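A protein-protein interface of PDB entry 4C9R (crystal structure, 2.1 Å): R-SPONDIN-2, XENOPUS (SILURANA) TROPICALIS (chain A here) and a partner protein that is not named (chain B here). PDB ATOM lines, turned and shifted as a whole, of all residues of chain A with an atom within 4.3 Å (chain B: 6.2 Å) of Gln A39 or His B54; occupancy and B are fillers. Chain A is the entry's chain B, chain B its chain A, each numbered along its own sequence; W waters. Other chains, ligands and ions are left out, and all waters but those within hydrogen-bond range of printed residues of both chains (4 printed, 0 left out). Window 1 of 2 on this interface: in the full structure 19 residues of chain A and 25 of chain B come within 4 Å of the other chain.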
ATOM      1  N   ASN A  19     -25.278  18.780 -26.930  1.00  0.00           N
ATOM      2  CA  ASN A  19     -24.539  17.545 -27.169  1.00  0.00           C
ATOM      3  C   ASN A  19     -23.813  16.972 -25.971  1.00  0.00           C
ATOM      4  O   ASN A  19     -23.108  15.977 -26.101  1.00  0.00           O
ATOM      5  CB  ASN A  19     -23.497  17.777 -28.229  1.00  0.00           C
ATOM      6  CG  ASN A  19     -24.067  17.796 -29.615  1.00  0.00           C
ATOM      7  OD1 ASN A  19     -24.835  16.928 -30.013  1.00  0.00           O
ATOM      8  ND2 ASN A  19     -23.699  18.783 -30.352  1.00  0.00           N
ATOM      9  N   CYS A  21     -20.900  16.520 -23.335  1.00  0.00           N
ATOM     10  CA  CYS A  21     -19.458  16.644 -23.543  1.00  0.00           C
ATOM     11  C   CYS A  21     -19.041  16.478 -24.996  1.00  0.00           C
ATOM     12  O   CYS A  21     -19.561  15.639 -25.721  1.00  0.00           O
ATOM     13  CB  CYS A  21     -18.681  15.628 -22.687  1.00  0.00           C
ATOM     14  SG  CYS A  21     -18.945  15.808 -20.884  1.00  0.00           S
ATOM     15  N   LEU A  22     -18.069  17.282 -25.394  1.00  0.00           N
ATOM     16  CA  LEU A  22     -17.451  17.218 -26.693  1.00  0.00           C
ATOM     17  C   LEU A  22     -15.998  16.723 -26.613  1.00  0.00           C
ATOM     18  O   LEU A  22     -15.559  16.011 -27.490  1.00  0.00           O
ATOM     19  CB  LEU A  22     -17.503  18.588 -27.342  1.00  0.00           C
ATOM     20  CG  LEU A  22     -18.924  19.147 -27.405  1.00  0.00           C
ATOM     21  CD1 LEU A  22     -18.889  20.646 -27.692  1.00  0.00           C
ATOM     22  CD2 LEU A  22     -19.694  18.359 -28.462  1.00  0.00           C
ATOM     23  N   PHE A  30     -15.076   8.821 -23.131  1.00  0.00           N
ATOM     24  CA  PHE A  30     -16.235   9.363 -23.801  1.00  0.00           C
ATOM     25  C   PHE A  30     -17.316   8.295 -24.052  1.00  0.00           C
ATOM     26  O   PHE A  30     -17.086   7.281 -24.747  1.00  0.00           O
ATOM     27  CB  PHE A  30     -15.807   9.945 -25.134  1.00  0.00           C
ATOM     28  CG  PHE A  30     -16.894  10.721 -25.821  1.00  0.00           C
ATOM     29  CD1 PHE A  30     -17.249  11.971 -25.352  1.00  0.00           C
ATOM     30  CD2 PHE A  30     -17.543  10.204 -26.931  1.00  0.00           C
ATOM     31  CE1 PHE A  30     -18.252  12.704 -25.979  1.00  0.00           C
ATOM     32  CE2 PHE A  30     -18.541  10.926 -27.572  1.00  0.00           C
ATOM     33  CZ  PHE A  30     -18.903  12.180 -27.086  1.00  0.00           C
ATOM     34  N   LEU A  32     -21.446   7.872 -25.198  1.00  0.00           N
ATOM     35  CA  LEU A  32     -22.650   8.442 -25.812  1.00  0.00           C
ATOM     36  C   LEU A  32     -23.915   7.910 -25.154  1.00  0.00           C
ATOM     37  O   LEU A  32     -24.269   6.749 -25.348  1.00  0.00           O
ATOM     38  CB  LEU A  32     -22.683   8.111 -27.305  1.00  0.00           C
ATOM     39  CG  LEU A  32     -21.775   9.029 -28.129  1.00  0.00           C
ATOM     40  CD1 LEU A  32     -21.735   8.672 -29.598  1.00  0.00           C
ATOM     41  CD2 LEU A  32     -22.200  10.467 -27.956  1.00  0.00           C
ATOM     42  N   ARG A  33     -24.589   8.754 -24.357  1.00  0.00           N
ATOM     43  CA  ARG A  33     -25.813   8.323 -23.688  1.00  0.00           C
ATOM     44  C   ARG A  33     -27.031   8.637 -24.577  1.00  0.00           C
ATOM     45  O   ARG A  33     -27.202   9.729 -25.053  1.00  0.00           O
ATOM     46  CB  ARG A  33     -25.967   8.972 -22.309  1.00  0.00           C
ATOM     47  CG  ARG A  33     -27.243   8.519 -21.575  1.00  0.00           C
ATOM     48  CD  ARG A  33     -27.266   8.827 -20.083  1.00  0.00           C
ATOM     49  NE  ARG A  33     -26.351   7.927 -19.355  1.00  0.00           N
ATOM     50  CZ  ARG A  33     -26.615   6.655 -19.011  1.00  0.00           C
ATOM     51  NH1 ARG A  33     -27.788   6.078 -19.295  1.00  0.00           N
ATOM     52  NH2 ARG A  33     -25.691   5.946 -18.363  1.00  0.00           N
ATOM     53  N   ARG A  34     -27.883   7.647 -24.744  1.00  0.00           N
ATOM     54  CA  ARG A  34     -29.102   7.707 -25.532  1.00  0.00           C
ATOM     55  C   ARG A  34     -30.244   7.903 -24.541  1.00  0.00           C
ATOM     56  O   ARG A  34     -30.407   7.076 -23.652  1.00  0.00           O
ATOM     57  CB  ARG A  34     -29.226   6.352 -26.271  1.00  0.00           C
ATOM     58  CG  ARG A  34     -30.325   6.168 -27.315  1.00  0.00           C
ATOM     59  CD  ARG A  34     -29.870   6.542 -28.717  1.00  0.00           C
ATOM     60  NE  ARG A  34     -30.408   7.846 -29.067  1.00  0.00           N
ATOM     61  CZ  ARG A  34     -30.030   8.591 -30.104  1.00  0.00           C
ATOM     62  NH1 ARG A  34     -29.089   8.187 -30.942  1.00  0.00           N
ATOM     63  NH2 ARG A  34     -30.610   9.765 -30.285  1.00  0.00           N
ATOM     64  N   MET A  37     -35.064  10.615 -27.804  1.00  0.00           N
ATOM     65  CA  MET A  37     -34.607  11.298 -29.033  1.00  0.00           C
ATOM     66  C   MET A  37     -33.170  11.782 -28.923  1.00  0.00           C
ATOM     67  O   MET A  37     -32.501  11.838 -29.926  1.00  0.00           O
ATOM     68  CB  MET A  37     -35.410  12.575 -29.346  1.00  0.00           C
ATOM     69  CG  MET A  37     -36.849  12.379 -29.783  1.00  0.00           C
ATOM     70  SD  MET A  37     -37.406  13.987 -30.385  1.00  0.00           S
ATOM     71  CE  MET A  37     -37.865  14.812 -28.868  1.00  0.00           C
ATOM     72  N   ARG A  38     -32.747  12.123 -27.700  1.00  0.00           N
ATOM     73  CA  ARG A  38     -31.440  12.690 -27.362  1.00  0.00           C
ATOM     74  C   ARG A  38     -30.276  11.726 -27.342  1.00  0.00           C
ATOM     75  O   ARG A  38     -30.414  10.568 -26.926  1.00  0.00           O
ATOM     76  CB  ARG A  38     -31.480  13.346 -25.977  1.00  0.00           C
ATOM     77  CG  ARG A  38     -32.647  14.305 -25.776  1.00  0.00           C
ATOM     78  CD  ARG A  38     -32.663  14.859 -24.357  1.00  0.00           C
ATOM     79  NE  ARG A  38     -31.406  15.565 -24.055  1.00  0.00           N
ATOM     80  CZ  ARG A  38     -30.906  15.739 -22.828  1.00  0.00           C
ATOM     81  NH1 ARG A  38     -31.530  15.232 -21.760  1.00  0.00           N
ATOM     82  NH2 ARG A  38     -29.761  16.401 -22.665  1.00  0.00           N
ATOM     83  N   GLN A  39     -29.115  12.235 -27.756  1.00  0.00           N
ATOM     84  CA  GLN A  39     -27.845  11.542 -27.629  1.00  0.00           C
ATOM     85  C   GLN A  39     -26.825  12.545 -27.100  1.00  0.00           C
ATOM     86  O   GLN A  39     -26.587  13.596 -27.749  1.00  0.00           O
ATOM     87  CB  GLN A  39     -27.383  10.956 -28.968  1.00  0.00           C
ATOM     88  CG  GLN A  39     -26.409   9.789 -28.798  1.00  0.00           C
ATOM     89  CD  GLN A  39     -25.788   9.297 -30.062  1.00  0.00           C
ATOM     90  OE1 GLN A  39     -25.440  10.072 -30.946  1.00  0.00           O
ATOM     91  NE2 GLN A  39     -25.574   7.962 -30.136  1.00  0.00           N
ATOM     92  N   TYR A  40     -26.271  12.299 -25.916  1.00  0.00           N
ATOM     93  CA  TYR A  40     -25.313  13.263 -25.385  1.00  0.00           C
ATOM     94  C   TYR A  40     -24.084  12.550 -24.856  1.00  0.00           C
ATOM     95  O   TYR A  40     -24.128  11.371 -24.504  1.00  0.00           O
ATOM     96  CB  TYR A  40     -25.930  14.307 -24.393  1.00  0.00           C
ATOM     97  CG  TYR A  40     -26.685  13.699 -23.274  1.00  0.00           C
ATOM     98  CD1 TYR A  40     -26.035  13.294 -22.115  1.00  0.00           C
ATOM     99  CD2 TYR A  40     -28.037  13.444 -23.394  1.00  0.00           C
ATOM    100  CE1 TYR A  40     -26.730  12.685 -21.104  1.00  0.00           C
ATOM    101  CE2 TYR A  40     -28.727  12.807 -22.392  1.00  0.00           C
ATOM    102  CZ  TYR A  40     -28.073  12.452 -21.247  1.00  0.00           C
ATOM    103  OH  TYR A  40     -28.780  11.813 -20.252  1.00  0.00           O
ATOM    104  N   GLY A  41     -22.982  13.275 -24.858  1.00  0.00           N
ATOM    105  CA  GLY A  41     -21.701  12.749 -24.444  1.00  0.00           C
ATOM    106  C   GLY A  41     -21.498  12.937 -22.957  1.00  0.00           C
ATOM    107  O   GLY A  41     -21.961  13.935 -22.384  1.00  0.00           O
ATOM    108  N   GLN B  52     -31.767  12.532 -32.528  1.00  0.00           N
ATOM    109  CA  GLN B  52     -30.532  13.289 -32.389  1.00  0.00           C
ATOM    110  C   GLN B  52     -29.350  12.351 -32.526  1.00  0.00           C
ATOM    111  O   GLN B  52     -29.398  11.241 -32.014  1.00  0.00           O
ATOM    112  CB  GLN B  52     -30.390  13.935 -31.040  1.00  0.00           C
ATOM    113  CG  GLN B  52     -29.095  14.774 -30.925  1.00  0.00           C
ATOM    114  CD  GLN B  52     -29.000  15.473 -29.601  1.00  0.00           C
ATOM    115  OE1 GLN B  52     -29.565  15.016 -28.620  1.00  0.00           O
ATOM    116  NE2 GLN B  52     -28.317  16.616 -29.573  1.00  0.00           N
ATOM    117  N   MET B  53     -28.319  12.816 -33.226  1.00  0.00           N
ATOM    118  CA  MET B  53     -27.021  12.150 -33.275  1.00  0.00           C
ATOM    119  C   MET B  53     -25.960  13.143 -32.892  1.00  0.00           C
ATOM    120  O   MET B  53     -25.896  14.235 -33.466  1.00  0.00           O
ATOM    121  CB  MET B  53     -26.716  11.623 -34.659  1.00  0.00           C
ATOM    122  CG  MET B  53     -27.734  10.619 -35.198  1.00  0.00           C
ATOM    123  SD  MET B  53     -27.836   9.054 -34.307  1.00  0.00           S
ATOM    124  CE  MET B  53     -26.278   8.290 -34.668  1.00  0.00           C
ATOM    125  N   HIS B  54     -25.182  12.792 -31.872  1.00  0.00           N
ATOM    126  CA  HIS B  54     -23.988  13.550 -31.467  1.00  0.00           C
ATOM    127  C   HIS B  54     -23.042  13.530 -32.682  1.00  0.00           C
ATOM    128  O   HIS B  54     -22.818  12.465 -33.258  1.00  0.00           O
ATOM    129  CB  HIS B  54     -23.365  12.858 -30.275  1.00  0.00           C
ATOM    130  CG  HIS B  54     -22.339  13.668 -29.551  1.00  0.00           C
ATOM    131  ND1 HIS B  54     -21.166  14.086 -30.138  1.00  0.00           N
ATOM    132  CD2 HIS B  54     -22.299  14.120 -28.271  1.00  0.00           C
ATOM    133  CE1 HIS B  54     -20.472  14.803 -29.274  1.00  0.00           C
ATOM    134  NE2 HIS B  54     -21.117  14.803 -28.125  1.00  0.00           N
ATOM    135  N   PRO B  55     -22.475  14.676 -33.068  1.00  0.00           N
ATOM    136  CA  PRO B  55     -21.615  14.678 -34.266  1.00  0.00           C
ATOM    137  C   PRO B  55     -20.445  13.694 -34.169  1.00  0.00           C
ATOM    138  O   PRO B  55     -20.095  13.070 -35.153  1.00  0.00           O
ATOM    139  CB  PRO B  55     -21.086  16.114 -34.342  1.00  0.00           C
ATOM    140  CG  PRO B  55     -21.511  16.790 -33.113  1.00  0.00           C
ATOM    141  CD  PRO B  55     -22.635  16.026 -32.509  1.00  0.00           C
ATOM    142  N   LEU B  56     -19.857  13.568 -32.990  1.00  0.00           N
ATOM    143  CA  LEU B  56     -18.685  12.707 -32.806  1.00  0.00           C
ATOM    144  C   LEU B  56     -18.964  11.228 -32.868  1.00  0.00           C
ATOM    145  O   LEU B  56     -18.058  10.446 -32.996  1.00  0.00           O
ATOM    146  CB  LEU B  56     -18.080  12.944 -31.458  1.00  0.00           C
ATOM    147  CG  LEU B  56     -17.306  14.237 -31.348  1.00  0.00           C
ATOM    148  CD1 LEU B  56     -17.008  14.501 -29.875  1.00  0.00           C
ATOM    149  CD2 LEU B  56     -16.020  14.051 -32.120  1.00  0.00           C
ATOM    150  N   GLY B  57     -20.214  10.850 -32.724  1.00  0.00           N
ATOM    151  CA  GLY B  57     -20.614   9.504 -32.915  1.00  0.00           C
ATOM    152  C   GLY B  57     -20.747   9.082 -34.374  1.00  0.00           C
ATOM    153  O   GLY B  57     -20.865   7.907 -34.622  1.00  0.00           O
ATOM    154  N   LEU B  58     -20.753  10.002 -35.339  1.00  0.00           N
ATOM    155  CA  LEU B  58     -20.888   9.597 -36.738  1.00  0.00           C
ATOM    156  C   LEU B  58     -19.494   9.432 -37.364  1.00  0.00           C
ATOM    157  O   LEU B  58     -18.862  10.396 -37.799  1.00  0.00           O
ATOM    158  CB  LEU B  58     -21.734  10.576 -37.513  1.00  0.00           C
ATOM    159  CG  LEU B  58     -23.179  10.646 -37.052  1.00  0.00           C
ATOM    160  CD1 LEU B  58     -23.813  11.951 -37.489  1.00  0.00           C
ATOM    161  CD2 LEU B  58     -23.942   9.450 -37.624  1.00  0.00           C
ATOM    162  N   TYR B  68     -30.906   0.958 -35.251  1.00  0.00           N
ATOM    163  CA  TYR B  68     -32.062   1.832 -35.125  1.00  0.00           C
ATOM    164  C   TYR B  68     -33.065   1.382 -36.138  1.00  0.00           C
ATOM    165  O   TYR B  68     -32.692   0.805 -37.147  1.00  0.00           O
ATOM    166  CB  TYR B  68     -31.719   3.279 -35.423  1.00  0.00           C
ATOM    167  CG  TYR B  68     -30.723   3.962 -34.500  1.00  0.00           C
ATOM    168  CD1 TYR B  68     -30.223   3.355 -33.367  1.00  0.00           C
ATOM    169  CD2 TYR B  68     -30.322   5.240 -34.774  1.00  0.00           C
ATOM    170  CE1 TYR B  68     -29.319   4.007 -32.542  1.00  0.00           C
ATOM    171  CE2 TYR B  68     -29.428   5.905 -33.964  1.00  0.00           C
ATOM    172  CZ  TYR B  68     -28.938   5.289 -32.843  1.00  0.00           C
ATOM    173  OH  TYR B  68     -28.057   5.988 -32.062  1.00  0.00           O
ATOM    174  N   VAL B  75     -30.960  14.437 -36.500  1.00  0.00           N
ATOM    175  CA  VAL B  75     -30.722  15.836 -36.153  1.00  0.00           C
ATOM    176  C   VAL B  75     -29.339  15.946 -35.554  1.00  0.00           C
ATOM    177  O   VAL B  75     -29.047  15.261 -34.611  1.00  0.00           O
ATOM    178  CB  VAL B  75     -31.775  16.363 -35.233  1.00  0.00           C
ATOM    179  CG1 VAL B  75     -31.454  17.808 -34.837  1.00  0.00           C
ATOM    180  CG2 VAL B  75     -33.102  16.276 -35.958  1.00  0.00           C
ATOM    181  N   VAL B  76     -28.460  16.684 -36.231  1.00  0.00           N
ATOM    182  CA  VAL B  76     -27.094  16.880 -35.810  1.00  0.00           C
ATOM    183  C   VAL B  76     -26.775  18.337 -35.580  1.00  0.00           C
ATOM    184  O   VAL B  76     -26.782  19.209 -36.492  1.00  0.00           O
ATOM    185  CB  VAL B  76     -26.102  16.326 -36.816  1.00  0.00           C
ATOM    186  CG1 VAL B  76     -24.680  16.363 -36.264  1.00  0.00           C
ATOM    187  CG2 VAL B  76     -26.509  14.921 -37.208  1.00  0.00           C
ATOM    188  N   LYS B  77     -26.489  18.603 -34.339  1.00  0.00           N
ATOM    189  CA  LYS B  77     -26.086  19.900 -33.941  1.00  0.00           C
ATOM    190  C   LYS B  77     -24.554  19.982 -34.026  1.00  0.00           C
ATOM    191  O   LYS B  77     -23.829  19.367 -33.253  1.00  0.00           O
ATOM    192  CB  LYS B  77     -26.628  20.179 -32.541  1.00  0.00           C
ATOM    193  CG  LYS B  77     -26.025  21.380 -31.849  1.00  0.00           C
ATOM    194  CD  LYS B  77     -26.610  22.656 -32.328  1.00  0.00           C
ATOM    195  CE  LYS B  77     -25.939  23.874 -31.654  1.00  0.00           C
ATOM    196  NZ  LYS B  77     -26.420  25.095 -32.367  1.00  0.00           N
ATOM    197  N   ARG B 101     -26.943   4.132 -41.718  1.00  0.00           N
ATOM    198  CA  ARG B 101     -27.508   3.579 -40.514  1.00  0.00           C
ATOM    199  C   ARG B 101     -29.058   3.707 -40.465  1.00  0.00           C
ATOM    200  O   ARG B 101     -29.662   3.519 -39.410  1.00  0.00           O
ATOM    201  CB  ARG B 101     -26.848   4.236 -39.303  1.00  0.00           C
ATOM    202  CG  ARG B 101     -25.398   3.773 -39.112  1.00  0.00           C
ATOM    203  CD  ARG B 101     -24.717   4.437 -37.929  1.00  0.00           C
ATOM    204  NE  ARG B 101     -25.348   4.170 -36.633  1.00  0.00           N
ATOM    205  CZ  ARG B 101     -25.074   4.851 -35.508  1.00  0.00           C
ATOM    206  NH1 ARG B 101     -24.176   5.838 -35.504  1.00  0.00           N
ATOM    207  NH2 ARG B 101     -25.698   4.545 -34.369  1.00  0.00           N
ATOM    208  N   VAL B 147     -36.109  18.697 -29.302  1.00  0.00           N
ATOM    209  CA  VAL B 147     -35.280  17.508 -29.130  1.00  0.00           C
ATOM    210  C   VAL B 147     -34.865  17.363 -27.663  1.00  0.00           C
ATOM    211  O   VAL B 147     -34.835  16.240 -27.114  1.00  0.00           O
ATOM    212  CB  VAL B 147     -34.016  17.578 -30.006  1.00  0.00           C
ATOM    213  CG1 VAL B 147     -33.069  16.446 -29.663  1.00  0.00           C
ATOM    214  CG2 VAL B 147     -34.376  17.509 -31.492  1.00  0.00           C
HETATM  215  O   HOH W   1     -29.744  16.457 -26.294  1.00  0.00           O
HETATM  216  O   HOH W   2     -23.783   9.883 -33.013  1.00  0.00           O
HETATM  217  O   HOH W   3     -24.128   6.942 -32.653  1.00  0.00           O
HETATM  218  O   HOH W   4     -26.283  16.594 -32.278  1.00  0.00           O
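NH2 of Arg A34 is in hydrogen-bond range of O of Gln B52. N of Gln B52 sits at hydrogen-bond distance from O of Met A37 (2.8 Å). The backbone NH of Gln A39 is in hydrogen-bond range of the side-chain amide oxygen of Gln B52 (2.9 Å). The side-chain sulfur (SD) of Met B53 sits at hydrogen-bond distance from the guanidinium group (NH1) of Arg A34, at 3.7 Å. O of Asn A19 sits close to NE2 of His B54. NE2 of His B54 is in hydrogen-bond range of O of Cys A21, 3.0 Å away. The side-chain amide oxygen (OE1) of Gln A39 sits at hydrogen-bond distance from the backbone NH (N) of His B54, at 2.9 Å. The side-chain hydroxyl of Tyr B68 sits at hydrogen-bond distance from the guanidinium group of Arg A34. The side-chain amide nitrogen of Asn A19 lies within hydrogen-bond range of the backbone carbonyl oxygen of Lys B77.
The backbone NH (N) of Met B53 lies within hydrogen-bond range of the backbone carbonyl oxygen (O) of Val B75. The backbone NH (N) of Leu B56 is in hydrogen-bond range of a ring nitrogen (ND1) of His B54 (3.2 Å). O of Asn A19 is in hydrogen-bond range of N of Gly A41, 3.0 Å away. The backbone NH (N) of Cys A21 is in hydrogen-bond range of the backbone carbonyl oxygen (O) of Gly A41 (3.0 Å). NH2 of Arg A34 lies within hydrogen-bond range of O of Met A37, at 2.8 Å. The guanidinium group (NH2) of Arg A34 sits close to the backbone carbonyl oxygen (O) of Arg A38 (3.5 Å).
Among the printed residues, merely in contact across the chains: Leu A22 with Leu B56 (3.2 Å), Arg A38 with Val B147 (3.2 Å), Arg A38 with Gln B52 (3.2 Å), Asn A19 with Pro B55 (3.4 Å), Gln A39 with Met B53 (3.5 Å), Asn A19 with Gln B52 (3.5 Å), Leu A32 with His B54 (3.5 Å), Gly A41 with His B54 (3.6 Å), Phe A30 with His B54 (3.6 Å), Leu A32 with Gly B57 (3.6 Å), Gln A39 with Tyr B68 (3.7 Å), Leu A22 with His B54 (3.7 Å) and Met A37 with Val B147 (3.7 Å).
Of the printed residues of chain B, Leu A32 touches His B54 (3.5 Å) and Gly B57 (3.6 Å). Printed residues of chain B within 4 Å of Arg A34: Gln B52 (2.6 Å), Met B53 (3.7 Å) and Tyr B68 (2.7 Å). Gln A39 touches just these residues of chain B: Gln B52, Met B53, His B54 and Tyr B68. Printed residues of chain B within 4 Å of Gly A41: His B54 (3.6 Å). Of chain A, only Asn A19 (3.0 Å), Cys A21 (3.0 Å), Leu A22 (3.7 Å), Phe A30 (3.6 Å), Leu A32 (3.5 Å), Gln A39 (2.9 Å) and Gly A41 (3.6 Å) come within 4 Å of His B54. Leu B58 touches none of the printed residues of chain A. Printed residues of chain A within 4 Å of Tyr B68: Arg A34 and Gln A39. Arg B101 touches none of the printed residues of chain A. Of the printed residues of chain A, Val B147 touches Met A37 and Arg A38. The nearest residue of chain B that does not touch Gln A39 is Gly B57 (5.2 Å). The nearest residue of chain A that does not touch His B54 is Tyr A40 (4.2 Å).
Of the 13 printed residues of chain B, 9 touch a printed residue of chain A. Printed residues of chain B that touch a printed residue of chain A: Gln B52, Met B53, His B54, Pro B55, Leu B56, Gly B57, Tyr B68, Lys B77 and Val B147. Hydrophobic or aromatic side chains of chain B within 4 Å of the printed part of chain A: Met B53, His B54, Pro B55, Leu B56 and Tyr B68. Of the 12 printed residues of chain A, 10 touch a printed residue of chain B. Hydrophobic or aromatic side chains of chain A that line the printed part of chain B: Leu A22, Phe A30, Leu A32 and Met A37. Along chain A the printed residues that touch a printed residue of chain B span positions 19 to 41.
Water W2 bridges the side-chain amide oxygen of Gln A39 and the backbone carbonyl oxygen of His B54. Water W4 lies within hydrogen-bond range of O of Met B53 (2.7 Å), OD1 of Asn A19 (2.7 Å), N of Lys B77 (2.9 Å) and NE2 of Gln B52 (3.4 Å). Water W1 lies within hydrogen-bond range of the side-chain amide oxygen (OE1) of Gln B52 (2.7 Å) and the guanidinium group (NE) of Arg A38 (2.9 Å). Water W3 lies within hydrogen-bond range of NH1 of Arg B101 and NE2 of Gln A39.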
